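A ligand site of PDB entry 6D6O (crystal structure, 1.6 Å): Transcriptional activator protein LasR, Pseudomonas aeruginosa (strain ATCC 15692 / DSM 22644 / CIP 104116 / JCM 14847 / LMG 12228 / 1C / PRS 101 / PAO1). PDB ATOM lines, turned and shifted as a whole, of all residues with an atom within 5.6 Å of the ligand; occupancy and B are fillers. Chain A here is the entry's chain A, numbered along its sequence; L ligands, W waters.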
ATOM      1  N   LEU A  36      27.213 -28.531  -1.179  1.00  0.00           N
ATOM      2  CA  LEU A  36      28.215 -27.645  -0.627  1.00  0.00           C
ATOM      3  C   LEU A  36      29.593 -28.285  -0.733  1.00  0.00           C
ATOM      4  O   LEU A  36      29.809 -29.410  -0.276  1.00  0.00           O
ATOM      5  CB  LEU A  36      27.893 -27.313   0.832  1.00  0.00           C
ATOM      6  CG  LEU A  36      28.607 -26.059   1.332  1.00  0.00           C
ATOM      7  CD1 LEU A  36      28.010 -24.831   0.660  1.00  0.00           C
ATOM      8  CD2 LEU A  36      28.475 -25.969   2.850  1.00  0.00           C
ATOM      9  N   PHE A  37      30.530 -27.562  -1.337  1.00  0.00           N
ATOM     10  CA  PHE A  37      31.910 -28.032  -1.465  1.00  0.00           C
ATOM     11  C   PHE A  37      32.732 -27.143  -0.555  1.00  0.00           C
ATOM     12  O   PHE A  37      32.751 -25.925  -0.741  1.00  0.00           O
ATOM     13  CB  PHE A  37      32.363 -27.910  -2.922  1.00  0.00           C
ATOM     14  CG  PHE A  37      33.817 -28.257  -3.165  1.00  0.00           C
ATOM     15  CD1 PHE A  37      34.818 -27.311  -2.980  1.00  0.00           C
ATOM     16  CD2 PHE A  37      34.162 -29.511  -3.656  1.00  0.00           C
ATOM     17  CE1 PHE A  37      36.158 -27.631  -3.234  1.00  0.00           C
ATOM     18  CE2 PHE A  37      35.493 -29.851  -3.908  1.00  0.00           C
ATOM     19  CZ  PHE A  37      36.490 -28.897  -3.712  1.00  0.00           C
ATOM     20  N   GLY A  38      33.349 -27.729   0.455  1.00  0.00           N
ATOM     21  CA  GLY A  38      34.149 -26.978   1.420  1.00  0.00           C
ATOM     22  C   GLY A  38      35.531 -27.577   1.507  1.00  0.00           C
ATOM     23  O   GLY A  38      35.690 -28.798   1.599  1.00  0.00           O
ATOM     24  N   LEU A  39      36.549 -26.726   1.456  1.00  0.00           N
ATOM     25  CA  LEU A  39      37.916 -27.206   1.422  1.00  0.00           C
ATOM     26  C   LEU A  39      38.818 -26.280   2.226  1.00  0.00           C
ATOM     27  O   LEU A  39      38.747 -25.049   2.097  1.00  0.00           O
ATOM     28  CB  LEU A  39      38.393 -27.307  -0.026  1.00  0.00           C
ATOM     29  CG  LEU A  39      39.654 -28.145  -0.272  1.00  0.00           C
ATOM     30  CD1 LEU A  39      39.402 -29.614   0.080  1.00  0.00           C
ATOM     31  CD2 LEU A  39      40.061 -27.995  -1.720  1.00  0.00           C
ATOM     32  N   LEU A  40      39.624 -26.893   3.100  1.00  0.00           N
ATOM     33  CA  LEU A  40      40.596 -26.181   3.922  1.00  0.00           C
ATOM     34  C   LEU A  40      41.997 -26.542   3.475  1.00  0.00           C
ATOM     35  O   LEU A  40      42.252 -27.675   3.081  1.00  0.00           O
ATOM     36  CB  LEU A  40      40.445 -26.582   5.397  1.00  0.00           C
ATOM     37  CG  LEU A  40      39.210 -26.166   6.200  1.00  0.00           C
ATOM     38  CD1 LEU A  40      39.130 -27.016   7.461  1.00  0.00           C
ATOM     39  CD2 LEU A  40      39.270 -24.701   6.584  1.00  0.00           C
ATOM     40  N   TYR A  47      38.428 -21.883  10.174  1.00  0.00           N
ATOM     41  CA  TYR A  47      37.789 -21.881   8.858  1.00  0.00           C
ATOM     42  C   TYR A  47      38.024 -20.585   8.093  1.00  0.00           C
ATOM     43  O   TYR A  47      37.394 -20.348   7.058  1.00  0.00           O
ATOM     44  CB  TYR A  47      36.288 -22.151   8.993  1.00  0.00           C
ATOM     45  CG  TYR A  47      35.978 -23.586   9.325  1.00  0.00           C
ATOM     46  CD1 TYR A  47      36.076 -24.064  10.632  1.00  0.00           C
ATOM     47  CD2 TYR A  47      35.609 -24.483   8.322  1.00  0.00           C
ATOM     48  CE1 TYR A  47      35.812 -25.384  10.935  1.00  0.00           C
ATOM     49  CE2 TYR A  47      35.343 -25.803   8.615  1.00  0.00           C
ATOM     50  CZ  TYR A  47      35.443 -26.254   9.911  1.00  0.00           C
ATOM     51  OH  TYR A  47      35.175 -27.574  10.194  1.00  0.00           O
ATOM     52  N   ILE A  52      34.641 -22.282   0.298  1.00  0.00           N
ATOM     53  CA  ILE A  52      33.322 -22.895   0.443  1.00  0.00           C
ATOM     54  C   ILE A  52      32.389 -22.365  -0.630  1.00  0.00           C
ATOM     55  O   ILE A  52      32.092 -21.168  -0.666  1.00  0.00           O
ATOM     56  CB  ILE A  52      32.717 -22.644   1.833  1.00  0.00           C
ATOM     57  CG1 ILE A  52      33.653 -23.160   2.916  1.00  0.00           C
ATOM     58  CG2 ILE A  52      31.325 -23.293   1.921  1.00  0.00           C
ATOM     59  CD1 ILE A  52      33.287 -22.767   4.332  1.00  0.00           C
ATOM     60  N   TYR A  56      23.678 -24.281  -1.112  1.00  0.00           N
ATOM     61  CA  TYR A  56      22.952 -24.297   0.160  1.00  0.00           C
ATOM     62  C   TYR A  56      22.353 -22.913   0.402  1.00  0.00           C
ATOM     63  O   TYR A  56      22.996 -21.910   0.093  1.00  0.00           O
ATOM     64  CB  TYR A  56      23.899 -24.612   1.321  1.00  0.00           C
ATOM     65  CG  TYR A  56      24.137 -26.087   1.583  1.00  0.00           C
ATOM     66  CD1 TYR A  56      23.900 -27.064   0.607  1.00  0.00           C
ATOM     67  CD2 TYR A  56      24.635 -26.502   2.817  1.00  0.00           C
ATOM     68  CE1 TYR A  56      24.126 -28.409   0.871  1.00  0.00           C
ATOM     69  CE2 TYR A  56      24.855 -27.853   3.092  1.00  0.00           C
ATOM     70  CZ  TYR A  56      24.600 -28.792   2.109  1.00  0.00           C
ATOM     71  OH  TYR A  56      24.823 -30.137   2.362  1.00  0.00           O
ATOM     72  N   TRP A  60      20.680 -20.817   6.051  1.00  0.00           N
ATOM     73  CA  TRP A  60      21.257 -22.002   6.666  1.00  0.00           C
ATOM     74  C   TRP A  60      22.781 -21.868   6.822  1.00  0.00           C
ATOM     75  O   TRP A  60      23.323 -22.201   7.884  1.00  0.00           O
ATOM     76  CB  TRP A  60      20.872 -23.255   5.861  1.00  0.00           C
ATOM     77  CG  TRP A  60      21.449 -24.528   6.375  1.00  0.00           C
ATOM     78  CD1 TRP A  60      22.226 -25.398   5.680  1.00  0.00           C
ATOM     79  CD2 TRP A  60      21.325 -25.079   7.704  1.00  0.00           C
ATOM     80  NE1 TRP A  60      22.576 -26.464   6.468  1.00  0.00           N
ATOM     81  CE2 TRP A  60      22.042 -26.291   7.713  1.00  0.00           C
ATOM     82  CE3 TRP A  60      20.663 -24.664   8.869  1.00  0.00           C
ATOM     83  CZ2 TRP A  60      22.128 -27.101   8.863  1.00  0.00           C
ATOM     84  CZ3 TRP A  60      20.754 -25.468  10.007  1.00  0.00           C
ATOM     85  CH2 TRP A  60      21.488 -26.676   9.984  1.00  0.00           C
ATOM     86  N   ARG A  61      23.463 -21.397   5.789  1.00  0.00           N
ATOM     87  CA  ARG A  61      24.901 -21.142   5.869  1.00  0.00           C
ATOM     88  C   ARG A  61      25.239 -20.214   7.040  1.00  0.00           C
ATOM     89  O   ARG A  61      26.136 -20.506   7.833  1.00  0.00           O
ATOM     90  CB  ARG A  61      25.424 -20.553   4.558  1.00  0.00           C
ATOM     91  CG  ARG A  61      25.420 -21.514   3.377  1.00  0.00           C
ATOM     92  CD  ARG A  61      26.588 -22.496   3.394  1.00  0.00           C
ATOM     93  NE  ARG A  61      27.854 -21.801   3.654  1.00  0.00           N
ATOM     94  CZ  ARG A  61      28.534 -21.120   2.741  1.00  0.00           C
ATOM     95  NH1 ARG A  61      28.107 -21.027   1.487  1.00  0.00           N
ATOM     96  NH2 ARG A  61      29.654 -20.511   3.101  1.00  0.00           N
ATOM     97  N   TYR A  64      24.363 -22.021  10.519  1.00  0.00           N
ATOM     98  CA  TYR A  64      25.332 -23.077  10.807  1.00  0.00           C
ATOM     99  C   TYR A  64      26.604 -22.481  11.372  1.00  0.00           C
ATOM    100  O   TYR A  64      27.164 -22.990  12.330  1.00  0.00           O
ATOM    101  CB  TYR A  64      25.600 -23.854   9.523  1.00  0.00           C
ATOM    102  CG  TYR A  64      26.510 -25.058   9.629  1.00  0.00           C
ATOM    103  CD1 TYR A  64      27.897 -24.896   9.730  1.00  0.00           C
ATOM    104  CD2 TYR A  64      26.004 -26.352   9.580  1.00  0.00           C
ATOM    105  CE1 TYR A  64      28.734 -25.999   9.808  1.00  0.00           C
ATOM    106  CE2 TYR A  64      26.838 -27.456   9.638  1.00  0.00           C
ATOM    107  CZ  TYR A  64      28.202 -27.276   9.763  1.00  0.00           C
ATOM    108  OH  TYR A  64      29.031 -28.372   9.823  1.00  0.00           O
ATOM    109  N   ASP A  65      27.058 -21.370  10.782  1.00  0.00           N
ATOM    110  CA  ASP A  65      28.225 -20.642  11.274  1.00  0.00           C
ATOM    111  C   ASP A  65      27.997 -20.039  12.663  1.00  0.00           C
ATOM    112  O   ASP A  65      28.766 -20.282  13.592  1.00  0.00           O
ATOM    113  CB  ASP A  65      28.613 -19.529  10.289  1.00  0.00           C
ATOM    114  CG  ASP A  65      29.131 -20.072   8.978  1.00  0.00           C
ATOM    115  OD1 ASP A  65      29.368 -21.295   8.863  1.00  0.00           O
ATOM    116  OD2 ASP A  65      29.303 -19.259   8.046  1.00  0.00           O
ATOM    117  N   ASP A  73      27.910 -31.125  14.045  1.00  0.00           N
ATOM    118  CA  ASP A  73      27.690 -31.876  12.810  1.00  0.00           C
ATOM    119  C   ASP A  73      28.547 -33.142  12.785  1.00  0.00           C
ATOM    120  O   ASP A  73      29.773 -33.065  12.701  1.00  0.00           O
ATOM    121  CB  ASP A  73      28.048 -30.942  11.660  1.00  0.00           C
ATOM    122  CG  ASP A  73      27.787 -31.543  10.289  1.00  0.00           C
ATOM    123  OD1 ASP A  73      27.539 -32.756  10.171  1.00  0.00           O
ATOM    124  OD2 ASP A  73      27.862 -30.761   9.323  1.00  0.00           O
ATOM    125  N   THR A  75      29.070 -35.254  10.529  1.00  0.00           N
ATOM    126  CA  THR A  75      29.770 -35.498   9.254  1.00  0.00           C
ATOM    127  C   THR A  75      31.160 -34.861   9.248  1.00  0.00           C
ATOM    128  O   THR A  75      32.069 -35.383   8.597  1.00  0.00           O
ATOM    129  CB  THR A  75      28.977 -35.004   8.023  1.00  0.00           C
ATOM    130  OG1 THR A  75      28.919 -33.579   8.022  1.00  0.00           O
ATOM    131  CG2 THR A  75      27.568 -35.589   8.011  1.00  0.00           C
ATOM    132  N   VAL A  76      31.310 -33.753   9.974  1.00  0.00           N
ATOM    133  CA  VAL A  76      32.590 -33.037  10.059  1.00  0.00           C
ATOM    134  C   VAL A  76      33.641 -33.906  10.748  1.00  0.00           C
ATOM    135  O   VAL A  76      34.710 -34.138  10.177  1.00  0.00           O
ATOM    136  CB  VAL A  76      32.450 -31.652  10.756  1.00  0.00           C
ATOM    137  CG1 VAL A  76      33.820 -31.007  10.947  1.00  0.00           C
ATOM    138  CG2 VAL A  76      31.546 -30.754   9.939  1.00  0.00           C
ATOM    139  N   CYS A  79      34.746 -36.763   8.584  1.00  0.00           N
ATOM    140  CA  CYS A  79      35.667 -36.393   7.497  1.00  0.00           C
ATOM    141  C   CYS A  79      37.126 -36.350   7.961  1.00  0.00           C
ATOM    142  O   CYS A  79      38.026 -36.646   7.188  1.00  0.00           O
ATOM    143  CB  CYS A  79      35.284 -35.069   6.866  1.00  0.00           C
ATOM    144  SG  CYS A  79      33.803 -35.106   5.837  1.00  0.00           S
ATOM    145  N   THR A  80      37.358 -35.984   9.217  1.00  0.00           N
ATOM    146  CA  THR A  80      38.708 -35.974   9.783  1.00  0.00           C
ATOM    147  C   THR A  80      39.289 -37.379   9.972  1.00  0.00           C
ATOM    148  O   THR A  80      40.495 -37.533  10.179  1.00  0.00           O
ATOM    149  CB  THR A  80      38.784 -35.209  11.136  1.00  0.00           C
ATOM    150  OG1 THR A  80      38.186 -35.996  12.177  1.00  0.00           O
ATOM    151  CG2 THR A  80      38.099 -33.860  11.048  1.00  0.00           C
ATOM    152  N   TRP A  88      23.533 -39.066   5.738  1.00  0.00           N
ATOM    153  CA  TRP A  88      22.891 -38.223   6.754  1.00  0.00           C
ATOM    154  C   TRP A  88      21.766 -38.964   7.454  1.00  0.00           C
ATOM    155  O   TRP A  88      20.708 -39.180   6.887  1.00  0.00           O
ATOM    156  CB  TRP A  88      22.296 -36.951   6.142  1.00  0.00           C
ATOM    157  CG  TRP A  88      23.245 -36.084   5.382  1.00  0.00           C
ATOM    158  CD1 TRP A  88      24.606 -36.208   5.306  1.00  0.00           C
ATOM    159  CD2 TRP A  88      22.899 -34.909   4.653  1.00  0.00           C
ATOM    160  NE1 TRP A  88      25.129 -35.198   4.531  1.00  0.00           N
ATOM    161  CE2 TRP A  88      24.103 -34.373   4.133  1.00  0.00           C
ATOM    162  CE3 TRP A  88      21.686 -34.257   4.383  1.00  0.00           C
ATOM    163  CZ2 TRP A  88      24.125 -33.223   3.338  1.00  0.00           C
ATOM    164  CZ3 TRP A  88      21.712 -33.108   3.607  1.00  0.00           C
ATOM    165  CH2 TRP A  88      22.921 -32.607   3.096  1.00  0.00           C
ATOM    166  N   ILE A  92      23.516 -41.024  13.117  1.00  0.00           N
ATOM    167  CA  ILE A  92      24.792 -40.330  13.355  1.00  0.00           C
ATOM    168  C   ILE A  92      24.668 -39.180  14.376  1.00  0.00           C
ATOM    169  O   ILE A  92      25.680 -38.613  14.806  1.00  0.00           O
ATOM    170  CB  ILE A  92      25.510 -39.872  12.051  1.00  0.00           C
ATOM    171  CG1 ILE A  92      24.664 -38.867  11.243  1.00  0.00           C
ATOM    172  CG2 ILE A  92      25.914 -41.086  11.214  1.00  0.00           C
ATOM    173  CD1 ILE A  92      25.184 -38.537   9.854  1.00  0.00           C
ATOM    174  N   PHE A 101      20.718 -29.820  15.649  1.00  0.00           N
ATOM    175  CA  PHE A 101      21.300 -29.703  14.311  1.00  0.00           C
ATOM    176  C   PHE A 101      20.449 -30.379  13.253  1.00  0.00           C
ATOM    177  O   PHE A 101      20.104 -29.762  12.244  1.00  0.00           O
ATOM    178  CB  PHE A 101      22.724 -30.254  14.278  1.00  0.00           C
ATOM    179  CG  PHE A 101      23.270 -30.447  12.878  1.00  0.00           C
ATOM    180  CD1 PHE A 101      23.652 -29.355  12.108  1.00  0.00           C
ATOM    181  CD2 PHE A 101      23.385 -31.732  12.338  1.00  0.00           C
ATOM    182  CE1 PHE A 101      24.132 -29.537  10.822  1.00  0.00           C
ATOM    183  CE2 PHE A 101      23.866 -31.914  11.051  1.00  0.00           C
ATOM    184  CZ  PHE A 101      24.259 -30.815  10.300  1.00  0.00           C
ATOM    185  N   PHE A 102      20.099 -31.641  13.479  1.00  0.00           N
ATOM    186  CA  PHE A 102      19.267 -32.367  12.519  1.00  0.00           C
ATOM    187  C   PHE A 102      17.898 -31.744  12.328  1.00  0.00           C
ATOM    188  O   PHE A 102      17.408 -31.640  11.197  1.00  0.00           O
ATOM    189  CB  PHE A 102      19.196 -33.859  12.848  1.00  0.00           C
ATOM    190  CG  PHE A 102      20.365 -34.630  12.325  1.00  0.00           C
ATOM    191  CD1 PHE A 102      21.384 -35.027  13.188  1.00  0.00           C
ATOM    192  CD2 PHE A 102      20.487 -34.913  10.972  1.00  0.00           C
ATOM    193  CE1 PHE A 102      22.478 -35.722  12.718  1.00  0.00           C
ATOM    194  CE2 PHE A 102      21.584 -35.616  10.482  1.00  0.00           C
ATOM    195  CZ  PHE A 102      22.576 -36.024  11.360  1.00  0.00           C
ATOM    196  N   ALA A 105      18.482 -28.541  10.285  1.00  0.00           N
ATOM    197  CA  ALA A 105      18.791 -28.905   8.899  1.00  0.00           C
ATOM    198  C   ALA A 105      17.518 -29.314   8.160  1.00  0.00           C
ATOM    199  O   ALA A 105      17.294 -28.879   7.028  1.00  0.00           O
ATOM    200  CB  ALA A 105      19.820 -30.021   8.841  1.00  0.00           C
ATOM    201  N   LEU A 110      17.027 -29.600   4.236  1.00  0.00           N
ATOM    202  CA  LEU A 110      18.156 -30.491   4.015  1.00  0.00           C
ATOM    203  C   LEU A 110      18.005 -31.692   4.937  1.00  0.00           C
ATOM    204  O   LEU A 110      18.521 -31.700   6.062  1.00  0.00           O
ATOM    205  CB  LEU A 110      19.462 -29.751   4.268  1.00  0.00           C
ATOM    206  CG  LEU A 110      19.705 -28.576   3.320  1.00  0.00           C
ATOM    207  CD1 LEU A 110      20.174 -27.356   4.089  1.00  0.00           C
ATOM    208  CD2 LEU A 110      20.691 -28.942   2.227  1.00  0.00           C
ATOM    209  N   THR A 115      27.694 -36.942   2.813  1.00  0.00           N
ATOM    210  CA  THR A 115      28.872 -36.080   2.834  1.00  0.00           C
ATOM    211  C   THR A 115      30.049 -36.961   2.432  1.00  0.00           C
ATOM    212  O   THR A 115      30.263 -38.039   3.001  1.00  0.00           O
ATOM    213  CB  THR A 115      29.040 -35.453   4.232  1.00  0.00           C
ATOM    214  OG1 THR A 115      27.946 -34.564   4.487  1.00  0.00           O
ATOM    215  CG2 THR A 115      30.354 -34.675   4.341  1.00  0.00           C
ATOM    216  N   LEU A 125      41.893 -30.570   3.240  1.00  0.00           N
ATOM    217  CA  LEU A 125      40.889 -31.324   3.979  1.00  0.00           C
ATOM    218  C   LEU A 125      39.537 -30.697   3.755  1.00  0.00           C
ATOM    219  O   LEU A 125      39.370 -29.489   3.908  1.00  0.00           O
ATOM    220  CB  LEU A 125      41.248 -31.323   5.469  1.00  0.00           C
ATOM    221  CG  LEU A 125      40.183 -31.769   6.491  1.00  0.00           C
ATOM    222  CD1 LEU A 125      39.851 -33.244   6.330  1.00  0.00           C
ATOM    223  CD2 LEU A 125      40.661 -31.464   7.906  1.00  0.00           C
ATOM    224  N   GLY A 126      38.552 -31.507   3.403  1.00  0.00           N
ATOM    225  CA  GLY A 126      37.255 -30.922   3.158  1.00  0.00           C
ATOM    226  C   GLY A 126      36.159 -31.942   2.981  1.00  0.00           C
ATOM    227  O   GLY A 126      36.287 -33.092   3.403  1.00  0.00           O
ATOM    228  N   ALA A 127      35.072 -31.479   2.374  1.00  0.00           N
ATOM    229  CA  ALA A 127      33.891 -32.310   2.200  1.00  0.00           C
ATOM    230  C   ALA A 127      33.079 -31.827   1.024  1.00  0.00           C
ATOM    231  O   ALA A 127      32.970 -30.624   0.780  1.00  0.00           O
ATOM    232  CB  ALA A 127      33.058 -32.257   3.471  1.00  0.00           C
ATOM    233  N   SER A 129      29.258 -32.162   0.283  1.00  0.00           N
ATOM    234  CA  SER A 129      27.976 -32.560   0.837  1.00  0.00           C
ATOM    235  C   SER A 129      26.874 -32.344  -0.193  1.00  0.00           C
ATOM    236  O   SER A 129      26.834 -31.333  -0.875  1.00  0.00           O
ATOM    237  CB  SER A 129      27.676 -31.767   2.096  1.00  0.00           C
ATOM    238  OG  SER A 129      28.603 -32.091   3.118  1.00  0.00           O
HETATM  239  C1  LIG L   1      35.973 -29.809   6.354  1.00  0.00           C
HETATM  240  C2  LIG L   1      35.218 -28.491   6.381  1.00  0.00           C
HETATM  241  C3  LIG L   1      34.276 -28.320   5.190  1.00  0.00           C
HETATM  242  C4  LIG L   1      32.980 -29.112   5.383  1.00  0.00           C
HETATM  243  C5  LIG L   1      31.749 -28.240   5.256  1.00  0.00           C
HETATM  244  O1  LIG L   1      31.504 -27.606   4.229  1.00  0.00           O
HETATM  245  O2  LIG L   1      30.844 -28.146   6.387  1.00  0.00           O
HETATM  246  C6  LIG L   1      29.659 -27.477   6.335  1.00  0.00           C
HETATM  247  C7  LIG L   1      29.628 -26.089   6.391  1.00  0.00           C
HETATM  248 BR1  LIG L   1      31.201 -25.064   6.522  1.00  0.00          BR
HETATM  249  C8  LIG L   1      28.433 -25.403   6.351  1.00  0.00           C
HETATM  250  C9  LIG L   1      27.259 -26.126   6.257  1.00  0.00           C
HETATM  251 BR2  LIG L   1      25.667 -25.173   6.196  1.00  0.00          BR
HETATM  252  C10 LIG L   1      27.267 -27.533   6.205  1.00  0.00           C
HETATM  253  C11 LIG L   1      28.472 -28.212   6.254  1.00  0.00           C
HETATM  254  C12 LIG L   1      28.566 -29.714   6.187  1.00  0.00           C
HETATM  255  N1  LIG L   1      27.352 -30.432   6.578  1.00  0.00           N
HETATM  256  C13 LIG L   1      26.294 -30.725   5.829  1.00  0.00           C
HETATM  257  O3  LIG L   1      26.199 -30.414   4.654  1.00  0.00           O
HETATM  258  C14 LIG L   1      25.171 -31.518   6.457  1.00  0.00           C
HETATM  259  C15 LIG L   1      23.870 -31.044   6.540  1.00  0.00           C
HETATM  260  N2  LIG L   1      23.503 -29.773   6.110  1.00  0.00           N
HETATM  261  O4  LIG L   1      22.233 -29.577   5.599  1.00  0.00           O
HETATM  262  O5  LIG L   1      24.256 -28.820   6.239  1.00  0.00           O
HETATM  263  C16 LIG L   1      25.471 -32.795   6.921  1.00  0.00           C
HETATM  264  C17 LIG L   1      24.476 -33.583   7.495  1.00  0.00           C
HETATM  265  C18 LIG L   1      23.169 -33.116   7.589  1.00  0.00           C
HETATM  266  C19 LIG L   1      22.874 -31.847   7.115  1.00  0.00           C
HETATM  267  C20 LIG L   1      35.560 -30.722   7.504  1.00  0.00           C
HETATM  268  C21 LIG L   1      36.761 -31.441   8.113  1.00  0.00           C
HETATM  269  C22 LIG L   1      37.238 -30.735   9.362  1.00  0.00           C
HETATM  270  O   HOH W   1      28.251 -21.936   6.480  1.00  0.00           O
HETATM  271  O   HOH W   2      30.427 -29.968   2.624  1.00  0.00           O
HETATM  272  O   HOH W   3      32.029 -27.169   8.826  1.00  0.00           O
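An oxygen (O3) of the ligand sits close to the side-chain hydroxyl (OG) of Ser 129 (3.3 Å).
The side-chain carboxylate (OD2) of Asp 73 sits at hydrogen-bond distance from a nitrogen (N1) of the ligand (2.8 Å).
An oxygen (O5) of the ligand sits at hydrogen-bond distance from the indole nitrogen (NE1) of Trp 60.
The side-chain hydroxyl (OH) of Tyr 56 is in hydrogen-bond range of an oxygen (O3) of the ligand, at 2.7 Å.
The backbone carbonyl oxygen of Ser 129 sits at hydrogen-bond distance from the backbone NH of Leu 36 (2.8 Å).
O of Leu 125 lies within hydrogen-bond range of N of Leu 40 (2.7 Å).
The backbone carbonyl oxygen of Thr 75 sits at hydrogen-bond distance from the side-chain sulfur of Cys 79.
The side-chain hydroxyl of Ser 129 lies within hydrogen-bond range of the side-chain hydroxyl of Thr 115, 2.9 Å away.
N of Ala 127 is in hydrogen-bond range of O of Gly 38 (2.9 Å).
The side-chain hydroxyl (OG1) of Thr 75 sits at hydrogen-bond distance from the side-chain carboxylate (OD1) of Asp 73.
NE1 of Trp 88 lies within hydrogen-bond range of OG1 of Thr 115 (2.9 Å).
The side-chain hydroxyl of Tyr 64 lies within hydrogen-bond range of the side-chain carboxylate of Asp 73.
Merely in contact with the ligand: Leu 36 (3.5 Å), Gly 38 (3.9 Å), Tyr 47 (3.5 Å), Ile 52 (3.8 Å), Arg 61 (3.98 Å), Tyr 64 (3.5 Å), Thr 75 (3.7 Å), Val 76 (3.8 Å), Thr 80 (3.7 Å), Trp 88 (3.4 Å), Phe 101 (3.6 Å), Ala 105 (3.95 Å), Leu 110 (3.1 Å), Thr 115 (3.9 Å), Leu 125 (3.8 Å), Gly 126 (3.6 Å) and Ala 127 (3.7 Å).
Hydrophobic or aromatic side chains that line the ligand: Leu 36, Tyr 47, Ile 52, Tyr 56, Trp 60, Tyr 64, Val 76, Trp 88, Phe 101, Ala 105, Leu 110, Leu 125 and Ala 127.
Within 4 Å of the ligand: Leu 36, Gly 38, Tyr 47, Ile 52, Tyr 56, Trp 60, Arg 61, Tyr 64, Asp 73, Thr 75, Val 76, Thr 80, Trp 88, Phe 101, Ala 105, Leu 110, Thr 115, Leu 125, Gly 126, Ala 127 and Ser 129.
The nearest printed residue that does not touch the ligand is Cys 79 (4.1 Å).
Water W3 lies within hydrogen-bond range of O2 of the ligand (2.9 Å), OH of Tyr 64 (3.4 Å) and OH of Tyr 47 (3.5 Å).
Water W1 lies within hydrogen-bond range of OD1 of Asp 65 (2.7 Å) and NE of Arg 61 (2.9 Å).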
